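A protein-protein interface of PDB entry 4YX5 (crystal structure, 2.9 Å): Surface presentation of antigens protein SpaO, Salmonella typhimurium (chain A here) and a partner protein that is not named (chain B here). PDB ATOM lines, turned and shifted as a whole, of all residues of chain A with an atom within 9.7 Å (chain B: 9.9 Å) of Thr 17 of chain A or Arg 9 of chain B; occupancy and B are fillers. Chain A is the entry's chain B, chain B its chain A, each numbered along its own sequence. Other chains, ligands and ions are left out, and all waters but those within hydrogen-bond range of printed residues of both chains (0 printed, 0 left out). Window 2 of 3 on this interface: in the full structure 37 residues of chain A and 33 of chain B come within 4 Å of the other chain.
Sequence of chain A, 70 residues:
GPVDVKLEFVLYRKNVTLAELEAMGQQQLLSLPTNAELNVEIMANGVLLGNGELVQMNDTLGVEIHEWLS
O of Lys 14 of chain A sits at hydrogen-bond distance from N of Leu 12 of chain B, at 2.9 Å. The backbone carbonyl oxygen (O) of Val 16 of chain A is in hydrogen-bond range of the backbone NH (N) of Trp 10 of chain B, 2.7 Å away.
Hydrophobic or aromatic side chains of chain A within 4 Å of the printed part of chain B: Val 16, Leu 18, Leu 21 and Met 24. Along chain A the printed residues that touch a printed residue of chain B span positions 14 to 24. Printed residues of chain B that touch a printed residue of chain A: Leu 8, Arg 9, Trp 10, Pro 11 and Leu 12. Along chain B the printed residues that touch a printed residue of chain A span positions 8 to 12. Among the printed residues, 14 pairs touch across the chains. Among the printed residues, no Asp or Glu carboxylate lies within 4 Å of a Lys or Arg side-chain nitrogen of the other chain.
Of the printed residues of chain B, Lys 14 of chain A touches Trp 10, Pro 11 and Leu 12. Of chain B, only Leu 8, Arg 9 and Trp 10 come within 4 Å of Thr 17 of chain A. No residue of chain B comes within 4 Å of Ala 19 of chain A. No residue of chain B comes within 4 Å of Glu 20 of chain A. Glu 22 of chain A touches none of the printed residues of chain B. Of chain A, only Val 16 and Thr 17 come within 4 Å of Leu 8 of chain B. Of chain A, only Val 16 and Thr 17 come within 4 Å of Arg 9 of chain B. Trp 10 of chain B touches just these residues of chain A: Lys 14, Asn 15, Val 16, Thr 17, Leu 18 and Leu 21. Of the printed residues of chain A, Pro 11 of chain B touches Lys 14 (3.9 Å) and Asn 15 (3.7 Å). Cys 46 of chain B touches none of the printed residues of chain A. The nearest printed residue of chain A that does not touch Pro 11 of chain B is Val 16 of chain A (4.9 Å).
O of Lys 14 of chain A touches O of Trp 10 of chain B (3.6 Å). Pro 11 of chain B touches Lys 14 of chain A (C to O, 3.9 Å). Asn 15 of chain A touches Trp 10 of chain B. O of Leu 8 of chain B touches O of Val 16 of chain A, at 3.96 Å. O of Val 16 of chain A touches CA of Arg 9 of chain B, 3.0 Å away. Thr 17 of chain A touches Arg 9 of chain B. Thr 17 of chain A touches Trp 10 of chain B (C to CZ3, 3.6 Å). CZ3 of Trp 10 of chain B touches N of Leu 18 of chain A, 3.1 Å away. CD2 of Leu 21 of chain A touches CE3 of Trp 10 of chain B (3.8 Å). Leu 12 of chain B touches Met 24 of chain A (CD1 to CE, 3.7 Å).
The backbone carbonyl oxygen of Pro 11 of chain B sits close to the side-chain sulfur of Cys 46 of chain B (3.6 Å). O of Met 7 of chain B sits close to NH2 of Arg 9 of chain B (3.5 Å). OE1 of Glu 20 of chain A sits at hydrogen-bond distance from N of Thr 17 of chain A (2.9 Å). The backbone NH (N) of Ala 19 of chain A sits close to the side-chain hydroxyl (OG1) of Thr 17 of chain A, at 3.2 Å. The side-chain carboxylate (OE2) of Glu 20 of chain A lies within salt-bridge range of the side-chain amino group (NZ) of Lys 14 of chain A, at 3.6 Å.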
ATOM      1  N   LYS A  14      -4.345   3.890 -23.750  1.00  0.00           N
ATOM      2  CA  LYS A  14      -3.883   4.878 -22.781  1.00  0.00           C
ATOM      3  C   LYS A  14      -2.835   4.295 -21.864  1.00  0.00           C
ATOM      4  O   LYS A  14      -3.011   3.193 -21.339  1.00  0.00           O
ATOM      5  CB  LYS A  14      -5.031   5.424 -21.939  1.00  0.00           C
ATOM      6  CG  LYS A  14      -4.749   6.809 -21.442  1.00  0.00           C
ATOM      7  CD  LYS A  14      -5.460   7.121 -20.156  1.00  0.00           C
ATOM      8  CE  LYS A  14      -4.784   8.297 -19.460  1.00  0.00           C
ATOM      9  NZ  LYS A  14      -5.503   8.672 -18.218  1.00  0.00           N
ATOM     10  N   ASN A  15      -1.738   5.033 -21.692  1.00  0.00           N
ATOM     11  CA  ASN A  15      -0.751   4.718 -20.670  1.00  0.00           C
ATOM     12  C   ASN A  15      -1.282   5.148 -19.326  1.00  0.00           C
ATOM     13  O   ASN A  15      -1.805   6.256 -19.161  1.00  0.00           O
ATOM     14  CB  ASN A  15       0.549   5.399 -20.958  1.00  0.00           C
ATOM     15  CG  ASN A  15       1.005   5.147 -22.351  1.00  0.00           C
ATOM     16  OD1 ASN A  15       1.286   4.010 -22.713  1.00  0.00           O
ATOM     17  ND2 ASN A  15       1.083   6.205 -23.159  1.00  0.00           N
ATOM     18  N   VAL A  16      -1.154   4.264 -18.354  1.00  0.00           N
ATOM     19  CA  VAL A  16      -1.923   4.428 -17.135  1.00  0.00           C
ATOM     20  C   VAL A  16      -1.027   4.231 -15.895  1.00  0.00           C
ATOM     21  O   VAL A  16      -0.075   3.439 -15.913  1.00  0.00           O
ATOM     22  CB  VAL A  16      -3.130   3.450 -17.158  1.00  0.00           C
ATOM     23  CG1 VAL A  16      -2.814   2.114 -16.444  1.00  0.00           C
ATOM     24  CG2 VAL A  16      -4.372   4.124 -16.664  1.00  0.00           C
ATOM     25  N   THR A  17      -1.306   4.999 -14.844  1.00  0.00           N
ATOM     26  CA  THR A  17      -0.520   4.943 -13.607  1.00  0.00           C
ATOM     27  C   THR A  17      -1.090   3.922 -12.633  1.00  0.00           C
ATOM     28  O   THR A  17      -2.241   3.524 -12.775  1.00  0.00           O
ATOM     29  CB  THR A  17      -0.498   6.280 -12.899  1.00  0.00           C
ATOM     30  OG1 THR A  17      -1.770   6.474 -12.279  1.00  0.00           O
ATOM     31  CG2 THR A  17      -0.253   7.413 -13.882  1.00  0.00           C
ATOM     32  N   LEU A  18      -0.316   3.511 -11.631  1.00  0.00           N
ATOM     33  CA  LEU A  18      -0.863   2.598 -10.623  1.00  0.00           C
ATOM     34  C   LEU A  18      -2.122   3.181  -9.966  1.00  0.00           C
ATOM     35  O   LEU A  18      -3.045   2.445  -9.605  1.00  0.00           O
ATOM     36  CB  LEU A  18       0.180   2.260  -9.555  1.00  0.00           C
ATOM     37  CG  LEU A  18      -0.283   1.143  -8.606  1.00  0.00           C
ATOM     38  CD1 LEU A  18      -0.468  -0.115  -9.388  1.00  0.00           C
ATOM     39  CD2 LEU A  18       0.687   0.881  -7.479  1.00  0.00           C
ATOM     40  N   ALA A  19      -2.164   4.504  -9.834  1.00  0.00           N
ATOM     41  CA  ALA A  19      -3.341   5.165  -9.301  1.00  0.00           C
ATOM     42  C   ALA A  19      -4.539   4.912 -10.208  1.00  0.00           C
ATOM     43  O   ALA A  19      -5.449   4.184  -9.837  1.00  0.00           O
ATOM     44  CB  ALA A  19      -3.091   6.651  -9.147  1.00  0.00           C
ATOM     45  N   GLU A  20      -4.517   5.489 -11.406  1.00  0.00           N
ATOM     46  CA  GLU A  20      -5.628   5.392 -12.355  1.00  0.00           C
ATOM     47  C   GLU A  20      -6.039   3.941 -12.633  1.00  0.00           C
ATOM     48  O   GLU A  20      -7.159   3.657 -13.048  1.00  0.00           O
ATOM     49  CB  GLU A  20      -5.244   6.075 -13.663  1.00  0.00           C
ATOM     50  CG  GLU A  20      -4.889   7.543 -13.542  1.00  0.00           C
ATOM     51  CD  GLU A  20      -3.933   8.014 -14.640  1.00  0.00           C
ATOM     52  OE1 GLU A  20      -3.128   7.193 -15.139  1.00  0.00           O
ATOM     53  OE2 GLU A  20      -3.991   9.210 -15.008  1.00  0.00           O
ATOM     54  N   LEU A  21      -5.115   3.022 -12.404  1.00  0.00           N
ATOM     55  CA  LEU A  21      -5.408   1.599 -12.497  1.00  0.00           C
ATOM     56  C   LEU A  21      -6.340   1.140 -11.378  1.00  0.00           C
ATOM     57  O   LEU A  21      -7.332   0.462 -11.632  1.00  0.00           O
ATOM     58  CB  LEU A  21      -4.115   0.805 -12.448  1.00  0.00           C
ATOM     59  CG  LEU A  21      -4.147  -0.476 -13.251  1.00  0.00           C
ATOM     60  CD1 LEU A  21      -4.801  -0.218 -14.589  1.00  0.00           C
ATOM     61  CD2 LEU A  21      -2.731  -0.972 -13.448  1.00  0.00           C
ATOM     62  N   GLU A  22      -6.005   1.504 -10.141  1.00  0.00           N
ATOM     63  CA  GLU A  22      -6.884   1.274  -9.003  1.00  0.00           C
ATOM     64  C   GLU A  22      -8.285   1.832  -9.286  1.00  0.00           C
ATOM     65  O   GLU A  22      -9.281   1.130  -9.129  1.00  0.00           O
ATOM     66  CB  GLU A  22      -6.299   1.907  -7.732  1.00  0.00           C
ATOM     67  N   ALA A  23      -8.351   3.079  -9.741  1.00  0.00           N
ATOM     68  CA  ALA A  23      -9.619   3.780  -9.953  1.00  0.00           C
ATOM     69  C   ALA A  23     -10.518   3.116 -10.991  1.00  0.00           C
ATOM     70  O   ALA A  23     -11.732   3.325 -11.008  1.00  0.00           O
ATOM     71  CB  ALA A  23      -9.356   5.226 -10.352  1.00  0.00           C
ATOM     72  N   MET A  24      -9.928   2.320 -11.866  1.00  0.00           N
ATOM     73  CA  MET A  24     -10.725   1.619 -12.849  1.00  0.00           C
ATOM     74  C   MET A  24     -11.184   0.248 -12.342  1.00  0.00           C
ATOM     75  O   MET A  24     -12.217  -0.264 -12.781  1.00  0.00           O
ATOM     76  CB  MET A  24      -9.944   1.478 -14.141  1.00  0.00           C
ATOM     77  CG  MET A  24     -10.034   2.688 -15.048  1.00  0.00           C
ATOM     78  SD  MET A  24      -9.224   2.310 -16.618  1.00  0.00           S
ATOM     79  CE  MET A  24      -7.592   1.886 -16.025  1.00  0.00           C
ATOM     80  N   GLY A  25     -10.421  -0.333 -11.414  1.00  0.00           N
ATOM     81  CA  GLY A  25     -10.785  -1.591 -10.771  1.00  0.00           C
ATOM     82  C   GLY A  25     -12.128  -1.496 -10.068  1.00  0.00           C
ATOM     83  O   GLY A  25     -12.797  -2.503  -9.819  1.00  0.00           O
ATOM     84  N   PRO B   5       9.510   2.113  -7.750  1.00  0.00           N
ATOM     85  CA  PRO B   5       9.374   3.450  -7.164  1.00  0.00           C
ATOM     86  C   PRO B   5       8.053   4.186  -7.448  1.00  0.00           C
ATOM     87  O   PRO B   5       7.984   5.374  -7.123  1.00  0.00           O
ATOM     88  CB  PRO B   5      10.555   4.199  -7.790  1.00  0.00           C
ATOM     89  CG  PRO B   5      11.629   3.071  -8.044  1.00  0.00           C
ATOM     90  CD  PRO B   5      10.934   1.731  -7.869  1.00  0.00           C
ATOM     91  N   LYS B   6       7.048   3.516  -8.018  1.00  0.00           N
ATOM     92  CA  LYS B   6       5.704   4.096  -8.206  1.00  0.00           C
ATOM     93  C   LYS B   6       5.637   5.261  -9.214  1.00  0.00           C
ATOM     94  O   LYS B   6       4.738   6.106  -9.170  1.00  0.00           O
ATOM     95  CB  LYS B   6       5.143   4.553  -6.858  1.00  0.00           C
ATOM     96  N   MET B   7       6.617   5.296 -10.111  1.00  0.00           N
ATOM     97  CA  MET B   7       6.615   6.145 -11.307  1.00  0.00           C
ATOM     98  C   MET B   7       6.244   5.265 -12.498  1.00  0.00           C
ATOM     99  O   MET B   7       6.685   5.476 -13.640  1.00  0.00           O
ATOM    100  CB  MET B   7       7.992   6.767 -11.533  1.00  0.00           C
ATOM    101  CG  MET B   7       9.123   5.716 -11.607  1.00  0.00           C
ATOM    102  SD  MET B   7      10.656   6.213 -12.460  1.00  0.00           S
ATOM    103  CE  MET B   7      10.866   7.869 -11.789  1.00  0.00           C
ATOM    104  N   LEU B   8       5.450   4.244 -12.209  1.00  0.00           N
ATOM    105  CA  LEU B   8       5.199   3.187 -13.167  1.00  0.00           C
ATOM    106  C   LEU B   8       4.016   3.495 -14.072  1.00  0.00           C
ATOM    107  O   LEU B   8       3.103   4.231 -13.679  1.00  0.00           O
ATOM    108  CB  LEU B   8       4.963   1.881 -12.428  1.00  0.00           C
ATOM    109  CG  LEU B   8       6.163   1.412 -11.613  1.00  0.00           C
ATOM    110  CD1 LEU B   8       5.704   0.412 -10.579  1.00  0.00           C
ATOM    111  CD2 LEU B   8       7.219   0.794 -12.517  1.00  0.00           C
ATOM    112  N   ARG B   9       4.050   2.940 -15.284  1.00  0.00           N
ATOM    113  CA  ARG B   9       2.929   3.033 -16.214  1.00  0.00           C
ATOM    114  C   ARG B   9       2.600   1.666 -16.785  1.00  0.00           C
ATOM    115  O   ARG B   9       3.481   0.830 -16.934  1.00  0.00           O
ATOM    116  CB  ARG B   9       3.229   3.991 -17.366  1.00  0.00           C
ATOM    117  CG  ARG B   9       3.682   5.414 -17.010  1.00  0.00           C
ATOM    118  CD  ARG B   9       2.655   6.242 -16.254  1.00  0.00           C
ATOM    119  NE  ARG B   9       3.191   6.482 -14.916  1.00  0.00           N
ATOM    120  CZ  ARG B   9       3.590   7.660 -14.452  1.00  0.00           C
ATOM    121  NH1 ARG B   9       3.465   8.750 -15.200  1.00  0.00           N
ATOM    122  NH2 ARG B   9       4.083   7.746 -13.217  1.00  0.00           N
ATOM    123  N   TRP B  10       1.328   1.447 -17.110  1.00  0.00           N
ATOM    124  CA  TRP B  10       0.901   0.254 -17.869  1.00  0.00           C
ATOM    125  C   TRP B  10       0.154   0.664 -19.125  1.00  0.00           C
ATOM    126  O   TRP B  10      -0.776   1.459 -19.051  1.00  0.00           O
ATOM    127  CB  TRP B  10       0.017  -0.658 -17.020  1.00  0.00           C
ATOM    128  CG  TRP B  10       0.736  -1.202 -15.858  1.00  0.00           C
ATOM    129  CD1 TRP B  10       1.336  -2.412 -15.773  1.00  0.00           C
ATOM    130  CD2 TRP B  10       0.984  -0.542 -14.620  1.00  0.00           C
ATOM    131  NE1 TRP B  10       1.925  -2.567 -14.544  1.00  0.00           N
ATOM    132  CE2 TRP B  10       1.724  -1.422 -13.811  1.00  0.00           C
ATOM    133  CE3 TRP B  10       0.649   0.715 -14.106  1.00  0.00           C
ATOM    134  CZ2 TRP B  10       2.140  -1.101 -12.526  1.00  0.00           C
ATOM    135  CZ3 TRP B  10       1.055   1.035 -12.824  1.00  0.00           C
ATOM    136  CH2 TRP B  10       1.790   0.131 -12.047  1.00  0.00           C
ATOM    137  N   PRO B  11       0.569   0.147 -20.287  1.00  0.00           N
ATOM    138  CA  PRO B  11      -0.119   0.551 -21.515  1.00  0.00           C
ATOM    139  C   PRO B  11      -1.359  -0.294 -21.776  1.00  0.00           C
ATOM    140  O   PRO B  11      -1.282  -1.504 -21.917  1.00  0.00           O
ATOM    141  CB  PRO B  11       0.943   0.332 -22.585  1.00  0.00           C
ATOM    142  CG  PRO B  11       1.731  -0.807 -22.072  1.00  0.00           C
ATOM    143  CD  PRO B  11       1.773  -0.644 -20.575  1.00  0.00           C
ATOM    144  N   LEU B  12      -2.510   0.347 -21.820  1.00  0.00           N
ATOM    145  CA  LEU B  12      -3.749  -0.387 -22.006  1.00  0.00           C
ATOM    146  C   LEU B  12      -4.299  -0.215 -23.402  1.00  0.00           C
ATOM    147  O   LEU B  12      -4.276   0.881 -23.975  1.00  0.00           O
ATOM    148  CB  LEU B  12      -4.800   0.063 -20.999  1.00  0.00           C
ATOM    149  CG  LEU B  12      -4.421  -0.024 -19.526  1.00  0.00           C
ATOM    150  CD1 LEU B  12      -5.623   0.345 -18.711  1.00  0.00           C
ATOM    151  CD2 LEU B  12      -3.920  -1.403 -19.143  1.00  0.00           C
ATOM    152  N   CYS B  46      -3.293  -5.550 -21.602  1.00  0.00           N
ATOM    153  CA  CYS B  46      -2.026  -4.973 -21.242  1.00  0.00           C
ATOM    154  C   CYS B  46      -0.985  -5.940 -21.723  1.00  0.00           C
ATOM    155  O   CYS B  46      -0.775  -6.975 -21.092  1.00  0.00           O
ATOM    156  CB  CYS B  46      -1.909  -4.751 -19.742  1.00  0.00           C
ATOM    157  SG  CYS B  46      -0.400  -3.857 -19.278  1.00  0.00           S
ATOM    158  N   TYR B  47      -0.344  -5.592 -22.838  1.00  0.00           N
ATOM    159  CA  TYR B  47       0.520  -6.505 -23.566  1.00  0.00           C
ATOM    160  C   TYR B  47      -0.336  -7.707 -23.959  1.00  0.00           C
ATOM    161  O   TYR B  47      -1.442  -7.537 -24.472  1.00  0.00           O
ATOM    162  CB  TYR B  47       1.736  -6.909 -22.728  1.00  0.00           C
ATOM    163  CG  TYR B  47       2.683  -5.766 -22.409  1.00  0.00           C
ATOM    164  CD1 TYR B  47       3.597  -5.318 -23.355  1.00  0.00           C
ATOM    165  CD2 TYR B  47       2.672  -5.143 -21.161  1.00  0.00           C
ATOM    166  CE1 TYR B  47       4.466  -4.283 -23.080  1.00  0.00           C
ATOM    167  CE2 TYR B  47       3.544  -4.103 -20.871  1.00  0.00           C
ATOM    168  CZ  TYR B  47       4.438  -3.680 -21.840  1.00  0.00           C
ATOM    169  OH  TYR B  47       5.312  -2.649 -21.585  1.00  0.00           O
